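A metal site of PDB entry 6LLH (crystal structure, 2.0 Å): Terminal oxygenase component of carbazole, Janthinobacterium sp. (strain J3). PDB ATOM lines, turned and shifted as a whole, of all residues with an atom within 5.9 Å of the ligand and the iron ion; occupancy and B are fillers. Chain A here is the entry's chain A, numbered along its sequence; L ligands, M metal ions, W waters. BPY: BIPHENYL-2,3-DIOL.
The nearest printed residue that does not touch the iron ion is Asn 177 (4.2 Å).
Merely in contact with the ligand: Leu 270 (2.9 Å), Val 272 (2.9 Å), Glu 284 (3.2 Å), Ile 262 (3.3 Å), Phe 329 (3.4 Å), Ala 259 (3.5 Å), Ile 184 (3.8 Å) and Phe 275 (3.9 Å).
Within 4 Å of the ligand: His 183, Ile 184, His 187, Ala 259, Ile 262, Leu 270, Val 272, Phe 275, Glu 284, Phe 329, Asn 330 and Asp 333.
The side-chain amide nitrogen (ND2) of Asn 330 lies within hydrogen-bond range of the side-chain carboxylate (OD2) of Asp 333 (2.8 Å).
The side-chain carboxylate (OD1) of Asp 333 sits close to the side-chain amide nitrogen (ND2) of Asn 177 (2.9 Å).
The backbone carbonyl oxygen of Phe 329 sits close to a ring nitrogen (ND1) of His 187.
N of Leu 270 lies within hydrogen-bond range of O of Glu 284, at 2.8 Å.
The backbone NH (N) of Val 272 sits at hydrogen-bond distance from the backbone carbonyl oxygen (O) of Gln 282 (2.8 Å).
OD1 of Asn 330 sits at hydrogen-bond distance from NE2 of Gln 282, 2.9 Å away.
The side-chain carboxylate (OE2) of Glu 284 sits at hydrogen-bond distance from the side-chain hydroxyl (OH) of Tyr 286 (2.6 Å).
The side-chain hydroxyl (OH) of Tyr 296 sits at hydrogen-bond distance from the side-chain carboxylate (OE1) of Glu 284 (2.8 Å).
ND2 of Asn 330 sits close to OK1 of the ligand (3.4 Å).
Water W3 lies within hydrogen-bond range of the side-chain carboxylate of Glu 284, the guanidinium group of Arg 337 and the side-chain carboxylate of Asp 333.
The iron ion is bound by OK1 of the ligand (2.0 Å), OD1 of Asp 333 (2.0 Å), OK2 of the ligand (2.1 Å), NE2 of His 183 (2.1 Å) and NE2 of His 187 (2.2 Å).
Slightly farther from the iron ion lies OD2 of Asp 333 (2.7 Å).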
ATOM      1  N   ASN A 177      12.349  -1.654  22.968  1.00  0.00           N
ATOM      2  CA  ASN A 177      11.382  -0.815  23.645  1.00  0.00           C
ATOM      3  C   ASN A 177      10.737  -1.551  24.825  1.00  0.00           C
ATOM      4  O   ASN A 177      10.693  -1.037  25.914  1.00  0.00           O
ATOM      5  CB  ASN A 177      10.352  -0.258  22.690  1.00  0.00           C
ATOM      6  CG  ASN A 177       9.303   0.513  23.457  1.00  0.00           C
ATOM      7  OD1 ASN A 177       9.562   1.656  23.825  1.00  0.00           O
ATOM      8  ND2 ASN A 177       8.175  -0.099  23.773  1.00  0.00           N
ATOM      9  N   GLY A 178      10.318  -2.803  24.614  1.00  0.00           N
ATOM     10  CA  GLY A 178       9.644  -3.593  25.637  1.00  0.00           C
ATOM     11  C   GLY A 178      10.515  -3.852  26.863  1.00  0.00           C
ATOM     12  O   GLY A 178      10.013  -3.778  28.011  1.00  0.00           O
ATOM     13  N   ASP A 180      13.219  -2.103  27.773  1.00  0.00           N
ATOM     14  CA  ASP A 180      13.929  -0.891  28.186  1.00  0.00           C
ATOM     15  C   ASP A 180      13.404  -0.366  29.526  1.00  0.00           C
ATOM     16  O   ASP A 180      12.266   0.129  29.585  1.00  0.00           O
ATOM     17  CB  ASP A 180      13.663   0.116  27.071  1.00  0.00           C
ATOM     18  CG  ASP A 180      14.328   1.453  27.195  1.00  0.00           C
ATOM     19  OD1 ASP A 180      14.623   1.864  28.355  1.00  0.00           O
ATOM     20  OD2 ASP A 180      14.447   2.095  26.104  1.00  0.00           O
ATOM     21  N   PRO A 181      14.196  -0.422  30.620  1.00  0.00           N
ATOM     22  CA  PRO A 181      13.703  -0.012  31.941  1.00  0.00           C
ATOM     23  C   PRO A 181      13.201   1.454  31.991  1.00  0.00           C
ATOM     24  O   PRO A 181      12.248   1.737  32.682  1.00  0.00           O
ATOM     25  CB  PRO A 181      14.947  -0.196  32.835  1.00  0.00           C
ATOM     26  CG  PRO A 181      15.752  -1.279  32.115  1.00  0.00           C
ATOM     27  CD  PRO A 181      15.588  -0.910  30.658  1.00  0.00           C
ATOM     28  N   HIS A 183      11.909   3.237  29.549  1.00  0.00           N
ATOM     29  CA  HIS A 183      10.830   3.591  28.662  1.00  0.00           C
ATOM     30  C   HIS A 183       9.479   3.784  29.391  1.00  0.00           C
ATOM     31  O   HIS A 183       8.549   4.275  28.815  1.00  0.00           O
ATOM     32  CB  HIS A 183      10.711   2.603  27.498  1.00  0.00           C
ATOM     33  CG  HIS A 183       9.695   1.542  27.708  1.00  0.00           C
ATOM     34  ND1 HIS A 183       9.918   0.464  28.490  1.00  0.00           N
ATOM     35  CD2 HIS A 183       8.433   1.441  27.252  1.00  0.00           C
ATOM     36  CE1 HIS A 183       8.862  -0.311  28.481  1.00  0.00           C
ATOM     37  NE2 HIS A 183       7.923   0.300  27.761  1.00  0.00           N
ATOM     38  N   ILE A 184       9.376   3.298  30.627  1.00  0.00           N
ATOM     39  CA  ILE A 184       8.229   3.468  31.528  1.00  0.00           C
ATOM     40  C   ILE A 184       7.731   4.917  31.565  1.00  0.00           C
ATOM     41  O   ILE A 184       6.584   5.139  31.749  1.00  0.00           O
ATOM     42  CB  ILE A 184       8.642   2.917  32.900  1.00  0.00           C
ATOM     43  CG1 ILE A 184       7.486   2.548  33.824  1.00  0.00           C
ATOM     44  CG2 ILE A 184       9.606   3.825  33.624  1.00  0.00           C
ATOM     45  CD1 ILE A 184       7.992   1.993  35.156  1.00  0.00           C
ATOM     46  N   ILE A 186       7.033   6.728  29.141  1.00  0.00           N
ATOM     47  CA  ILE A 186       6.007   6.950  28.121  1.00  0.00           C
ATOM     48  C   ILE A 186       4.625   6.521  28.615  1.00  0.00           C
ATOM     49  O   ILE A 186       3.640   6.870  28.004  1.00  0.00           O
ATOM     50  CB  ILE A 186       6.257   6.246  26.756  1.00  0.00           C
ATOM     51  CG1 ILE A 186       5.961   4.743  26.835  1.00  0.00           C
ATOM     52  CG2 ILE A 186       7.630   6.575  26.194  1.00  0.00           C
ATOM     53  CD1 ILE A 186       6.172   3.986  25.511  1.00  0.00           C
ATOM     54  N   HIS A 187       4.568   5.744  29.691  1.00  0.00           N
ATOM     55  CA  HIS A 187       3.322   5.202  30.205  1.00  0.00           C
ATOM     56  C   HIS A 187       2.725   6.052  31.326  1.00  0.00           C
ATOM     57  O   HIS A 187       1.726   5.629  31.939  1.00  0.00           O
ATOM     58  CB  HIS A 187       3.595   3.787  30.700  1.00  0.00           C
ATOM     59  CG  HIS A 187       3.856   2.820  29.584  1.00  0.00           C
ATOM     60  ND1 HIS A 187       2.968   2.639  28.549  1.00  0.00           N
ATOM     61  CD2 HIS A 187       4.906   2.005  29.335  1.00  0.00           C
ATOM     62  CE1 HIS A 187       3.459   1.728  27.725  1.00  0.00           C
ATOM     63  NE2 HIS A 187       4.625   1.329  28.170  1.00  0.00           N
ATOM     64  N   LEU A 200       3.784   3.533  39.677  1.00  0.00           N
ATOM     65  CA  LEU A 200       4.582   3.557  38.447  1.00  0.00           C
ATOM     66  C   LEU A 200       5.544   4.715  38.541  1.00  0.00           C
ATOM     67  O   LEU A 200       5.187   5.874  38.409  1.00  0.00           O
ATOM     68  CB  LEU A 200       3.702   3.696  37.201  1.00  0.00           C
ATOM     69  CG  LEU A 200       4.399   3.338  35.880  1.00  0.00           C
ATOM     70  CD1 LEU A 200       4.492   1.838  35.740  1.00  0.00           C
ATOM     71  CD2 LEU A 200       3.655   3.930  34.698  1.00  0.00           C
ATOM     72  N   VAL A 258       3.280  -3.856  40.357  1.00  0.00           N
ATOM     73  CA  VAL A 258       3.296  -4.762  39.214  1.00  0.00           C
ATOM     74  C   VAL A 258       4.713  -4.772  38.628  1.00  0.00           C
ATOM     75  O   VAL A 258       5.588  -3.935  38.997  1.00  0.00           O
ATOM     76  CB  VAL A 258       2.201  -4.392  38.189  1.00  0.00           C
ATOM     77  CG1 VAL A 258       0.803  -4.630  38.744  1.00  0.00           C
ATOM     78  CG2 VAL A 258       2.341  -2.967  37.652  1.00  0.00           C
ATOM     79  N   ALA A 259       4.985  -5.745  37.746  1.00  0.00           N
ATOM     80  CA  ALA A 259       6.206  -5.734  36.999  1.00  0.00           C
ATOM     81  C   ALA A 259       7.399  -5.885  37.962  1.00  0.00           C
ATOM     82  O   ALA A 259       8.401  -5.226  37.804  1.00  0.00           O
ATOM     83  CB  ALA A 259       6.265  -4.464  36.174  1.00  0.00           C
ATOM     84  N   ILE A 262      10.805  -8.724  34.938  1.00  0.00           N
ATOM     85  CA  ILE A 262      10.735  -8.448  33.537  1.00  0.00           C
ATOM     86  C   ILE A 262      11.911  -9.204  32.911  1.00  0.00           C
ATOM     87  O   ILE A 262      13.055  -9.088  33.383  1.00  0.00           O
ATOM     88  CB  ILE A 262      10.836  -6.944  33.251  1.00  0.00           C
ATOM     89  CG1 ILE A 262       9.846  -6.165  34.109  1.00  0.00           C
ATOM     90  CG2 ILE A 262      10.657  -6.682  31.756  1.00  0.00           C
ATOM     91  CD1 ILE A 262       9.906  -4.695  33.868  1.00  0.00           C
ATOM     92  N   LEU A 270       8.869 -11.136  25.569  1.00  0.00           N
ATOM     93  CA  LEU A 270       8.953 -10.474  26.850  1.00  0.00           C
ATOM     94  C   LEU A 270       7.955 -11.102  27.818  1.00  0.00           C
ATOM     95  O   LEU A 270       6.828 -11.420  27.441  1.00  0.00           O
ATOM     96  CB  LEU A 270       8.629  -8.991  26.653  1.00  0.00           C
ATOM     97  CG  LEU A 270       8.938  -8.105  27.862  1.00  0.00           C
ATOM     98  CD1 LEU A 270      10.430  -7.835  28.003  1.00  0.00           C
ATOM     99  CD2 LEU A 270       8.229  -6.781  27.743  1.00  0.00           C
ATOM    100  N   VAL A 272       6.370 -10.079  31.635  1.00  0.00           N
ATOM    101  CA  VAL A 272       6.262  -9.099  32.718  1.00  0.00           C
ATOM    102  C   VAL A 272       5.355  -9.734  33.771  1.00  0.00           C
ATOM    103  O   VAL A 272       4.200 -10.070  33.467  1.00  0.00           O
ATOM    104  CB  VAL A 272       5.692  -7.766  32.224  1.00  0.00           C
ATOM    105  CG1 VAL A 272       5.705  -6.640  33.255  1.00  0.00           C
ATOM    106  CG2 VAL A 272       6.437  -7.342  30.966  1.00  0.00           C
ATOM    107  N   PHE A 275       1.535  -8.550  35.784  1.00  0.00           N
ATOM    108  CA  PHE A 275       1.031  -7.485  34.971  1.00  0.00           C
ATOM    109  C   PHE A 275      -0.172  -7.983  34.175  1.00  0.00           C
ATOM    110  O   PHE A 275      -0.108  -9.087  33.633  1.00  0.00           O
ATOM    111  CB  PHE A 275       2.133  -6.985  34.032  1.00  0.00           C
ATOM    112  CG  PHE A 275       1.901  -5.611  33.505  1.00  0.00           C
ATOM    113  CD1 PHE A 275       2.278  -4.503  34.255  1.00  0.00           C
ATOM    114  CD2 PHE A 275       1.291  -5.407  32.279  1.00  0.00           C
ATOM    115  CE1 PHE A 275       1.987  -3.234  33.816  1.00  0.00           C
ATOM    116  CE2 PHE A 275       1.012  -4.136  31.834  1.00  0.00           C
ATOM    117  CZ  PHE A 275       1.364  -3.045  32.604  1.00  0.00           C
ATOM    118  N   GLN A 282       1.975 -10.928  31.741  1.00  0.00           N
ATOM    119  CA  GLN A 282       1.901 -10.627  30.312  1.00  0.00           C
ATOM    120  C   GLN A 282       3.108 -11.287  29.631  1.00  0.00           C
ATOM    121  O   GLN A 282       4.240 -11.204  30.114  1.00  0.00           O
ATOM    122  CB  GLN A 282       1.881  -9.132  30.057  1.00  0.00           C
ATOM    123  CG  GLN A 282       1.721  -8.727  28.578  1.00  0.00           C
ATOM    124  CD  GLN A 282       1.173  -7.335  28.462  1.00  0.00           C
ATOM    125  OE1 GLN A 282       0.538  -6.854  29.405  1.00  0.00           O
ATOM    126  NE2 GLN A 282       1.442  -6.651  27.345  1.00  0.00           N
ATOM    127  N   GLU A 284       4.548 -11.212  25.638  1.00  0.00           N
ATOM    128  CA  GLU A 284       4.358 -10.627  24.319  1.00  0.00           C
ATOM    129  C   GLU A 284       5.565 -10.912  23.406  1.00  0.00           C
ATOM    130  O   GLU A 284       6.701 -10.756  23.780  1.00  0.00           O
ATOM    131  CB  GLU A 284       4.074  -9.134  24.398  1.00  0.00           C
ATOM    132  CG  GLU A 284       5.112  -8.313  25.132  1.00  0.00           C
ATOM    133  CD  GLU A 284       4.646  -6.869  25.207  1.00  0.00           C
ATOM    134  OE1 GLU A 284       3.441  -6.703  25.385  1.00  0.00           O
ATOM    135  OE2 GLU A 284       5.440  -5.925  24.956  1.00  0.00           O
ATOM    136  N   TYR A 286       7.401 -10.339  19.542  1.00  0.00           N
ATOM    137  CA  TYR A 286       7.585  -9.426  18.466  1.00  0.00           C
ATOM    138  C   TYR A 286       8.153 -10.216  17.288  1.00  0.00           C
ATOM    139  O   TYR A 286       9.370 -10.492  17.204  1.00  0.00           O
ATOM    140  CB  TYR A 286       8.483  -8.268  18.882  1.00  0.00           C
ATOM    141  CG  TYR A 286       8.322  -7.804  20.310  1.00  0.00           C
ATOM    142  CD1 TYR A 286       7.352  -6.902  20.673  1.00  0.00           C
ATOM    143  CD2 TYR A 286       9.132  -8.320  21.304  1.00  0.00           C
ATOM    144  CE1 TYR A 286       7.202  -6.507  21.993  1.00  0.00           C
ATOM    145  CE2 TYR A 286       8.991  -7.937  22.634  1.00  0.00           C
ATOM    146  CZ  TYR A 286       8.016  -7.031  22.975  1.00  0.00           C
ATOM    147  OH  TYR A 286       7.890  -6.587  24.270  1.00  0.00           O
ATOM    148  N   TYR A 296       2.844  -8.031  16.621  1.00  0.00           N
ATOM    149  CA  TYR A 296       2.812  -7.772  18.066  1.00  0.00           C
ATOM    150  C   TYR A 296       1.788  -8.743  18.685  1.00  0.00           C
ATOM    151  O   TYR A 296       0.543  -8.470  18.720  1.00  0.00           O
ATOM    152  CB  TYR A 296       2.508  -6.294  18.306  1.00  0.00           C
ATOM    153  CG  TYR A 296       2.479  -5.860  19.749  1.00  0.00           C
ATOM    154  CD1 TYR A 296       3.296  -6.436  20.689  1.00  0.00           C
ATOM    155  CD2 TYR A 296       1.620  -4.868  20.182  1.00  0.00           C
ATOM    156  CE1 TYR A 296       3.298  -6.049  22.024  1.00  0.00           C
ATOM    157  CE2 TYR A 296       1.614  -4.448  21.501  1.00  0.00           C
ATOM    158  CZ  TYR A 296       2.433  -5.044  22.437  1.00  0.00           C
ATOM    159  OH  TYR A 296       2.396  -4.680  23.768  1.00  0.00           O
ATOM    160  N   PHE A 329      -2.625   0.569  27.779  1.00  0.00           N
ATOM    161  CA  PHE A 329      -1.243   0.728  28.163  1.00  0.00           C
ATOM    162  C   PHE A 329      -0.293   0.603  26.937  1.00  0.00           C
ATOM    163  O   PHE A 329       0.522   1.485  26.699  1.00  0.00           O
ATOM    164  CB  PHE A 329      -0.913  -0.260  29.267  1.00  0.00           C
ATOM    165  CG  PHE A 329       0.411  -0.063  29.940  1.00  0.00           C
ATOM    166  CD1 PHE A 329       0.525   0.774  31.036  1.00  0.00           C
ATOM    167  CD2 PHE A 329       1.530  -0.786  29.528  1.00  0.00           C
ATOM    168  CE1 PHE A 329       1.720   0.897  31.703  1.00  0.00           C
ATOM    169  CE2 PHE A 329       2.731  -0.654  30.209  1.00  0.00           C
ATOM    170  CZ  PHE A 329       2.813   0.157  31.312  1.00  0.00           C
ATOM    171  N   ASN A 330      -0.408  -0.495  26.172  1.00  0.00           N
ATOM    172  CA  ASN A 330       0.626  -0.835  25.140  1.00  0.00           C
ATOM    173  C   ASN A 330       0.453  -0.012  23.869  1.00  0.00           C
ATOM    174  O   ASN A 330       1.341  -0.023  23.012  1.00  0.00           O
ATOM    175  CB  ASN A 330       0.694  -2.352  24.864  1.00  0.00           C
ATOM    176  CG  ASN A 330       1.160  -3.178  26.049  1.00  0.00           C
ATOM    177  OD1 ASN A 330       0.455  -4.095  26.465  1.00  0.00           O
ATOM    178  ND2 ASN A 330       2.346  -2.877  26.595  1.00  0.00           N
ATOM    179  N   ASP A 333       3.401   2.048  23.317  1.00  0.00           N
ATOM    180  CA  ASP A 333       4.586   1.282  22.901  1.00  0.00           C
ATOM    181  C   ASP A 333       4.650   1.218  21.371  1.00  0.00           C
ATOM    182  O   ASP A 333       5.730   1.337  20.783  1.00  0.00           O
ATOM    183  CB  ASP A 333       4.604  -0.145  23.425  1.00  0.00           C
ATOM    184  CG  ASP A 333       4.824  -0.188  24.917  1.00  0.00           C
ATOM    185  OD1 ASP A 333       5.818   0.371  25.358  1.00  0.00           O
ATOM    186  OD2 ASP A 333       3.969  -0.765  25.605  1.00  0.00           O
ATOM    187  N   ARG A 337       7.851   2.646  19.154  1.00  0.00           N
ATOM    188  CA  ARG A 337       8.605   1.775  18.268  1.00  0.00           C
ATOM    189  C   ARG A 337       8.684   2.430  16.896  1.00  0.00           C
ATOM    190  O   ARG A 337       9.700   2.441  16.298  1.00  0.00           O
ATOM    191  CB  ARG A 337       7.923   0.441  17.972  1.00  0.00           C
ATOM    192  CG  ARG A 337       7.784  -0.479  19.153  1.00  0.00           C
ATOM    193  CD  ARG A 337       6.906  -1.636  18.742  1.00  0.00           C
ATOM    194  NE  ARG A 337       6.434  -2.191  19.975  1.00  0.00           N
ATOM    195  CZ  ARG A 337       5.431  -3.048  20.098  1.00  0.00           C
ATOM    196  NH1 ARG A 337       4.881  -3.651  19.041  1.00  0.00           N
ATOM    197  NH2 ARG A 337       4.947  -3.240  21.305  1.00  0.00           N
HETATM  198  CK1 BPY L   1       6.460  -4.515  30.128  1.00  0.00           C
HETATM  199  CK2 BPY L   1       6.380  -3.187  30.369  1.00  0.00           C
HETATM  200  CK3 BPY L   1       6.111  -2.372  29.188  1.00  0.00           C
HETATM  201  CK4 BPY L   1       5.918  -2.946  27.868  1.00  0.00           C
HETATM  202  CK5 BPY L   1       5.988  -4.290  27.706  1.00  0.00           C
HETATM  203  CK6 BPY L   1       6.257  -5.035  28.839  1.00  0.00           C
HETATM  204  CK7 BPY L   1       6.572  -2.655  31.742  1.00  0.00           C
HETATM  205  CK8 BPY L   1       7.854  -2.571  32.242  1.00  0.00           C
HETATM  206  CK9 BPY L   1       8.063  -2.025  33.507  1.00  0.00           C
HETATM  207  CKA BPY L   1       7.001  -1.590  34.311  1.00  0.00           C
HETATM  208  CKB BPY L   1       5.692  -1.674  33.794  1.00  0.00           C
HETATM  209  CKC BPY L   1       5.497  -2.215  32.513  1.00  0.00           C
HETATM  210  OK1 BPY L   1       5.684  -2.077  26.899  1.00  0.00           O
HETATM  211  OK2 BPY L   1       5.997  -1.054  29.207  1.00  0.00           O
HETATM  212 FE    FE M   1       5.932  -0.166  27.313  1.00  0.00          FE
HETATM  213  O   HOH W   1      10.544  -2.847  30.532  1.00  0.00           O
HETATM  214  O   HOH W   2       3.290  -4.377  29.637  1.00  0.00           O
HETATM  215  O   HOH W   3       5.637  -3.495  24.399  1.00  0.00           O
HETATM  216  O   HOH W   4       9.839  -1.917  35.668  1.00  0.00           O
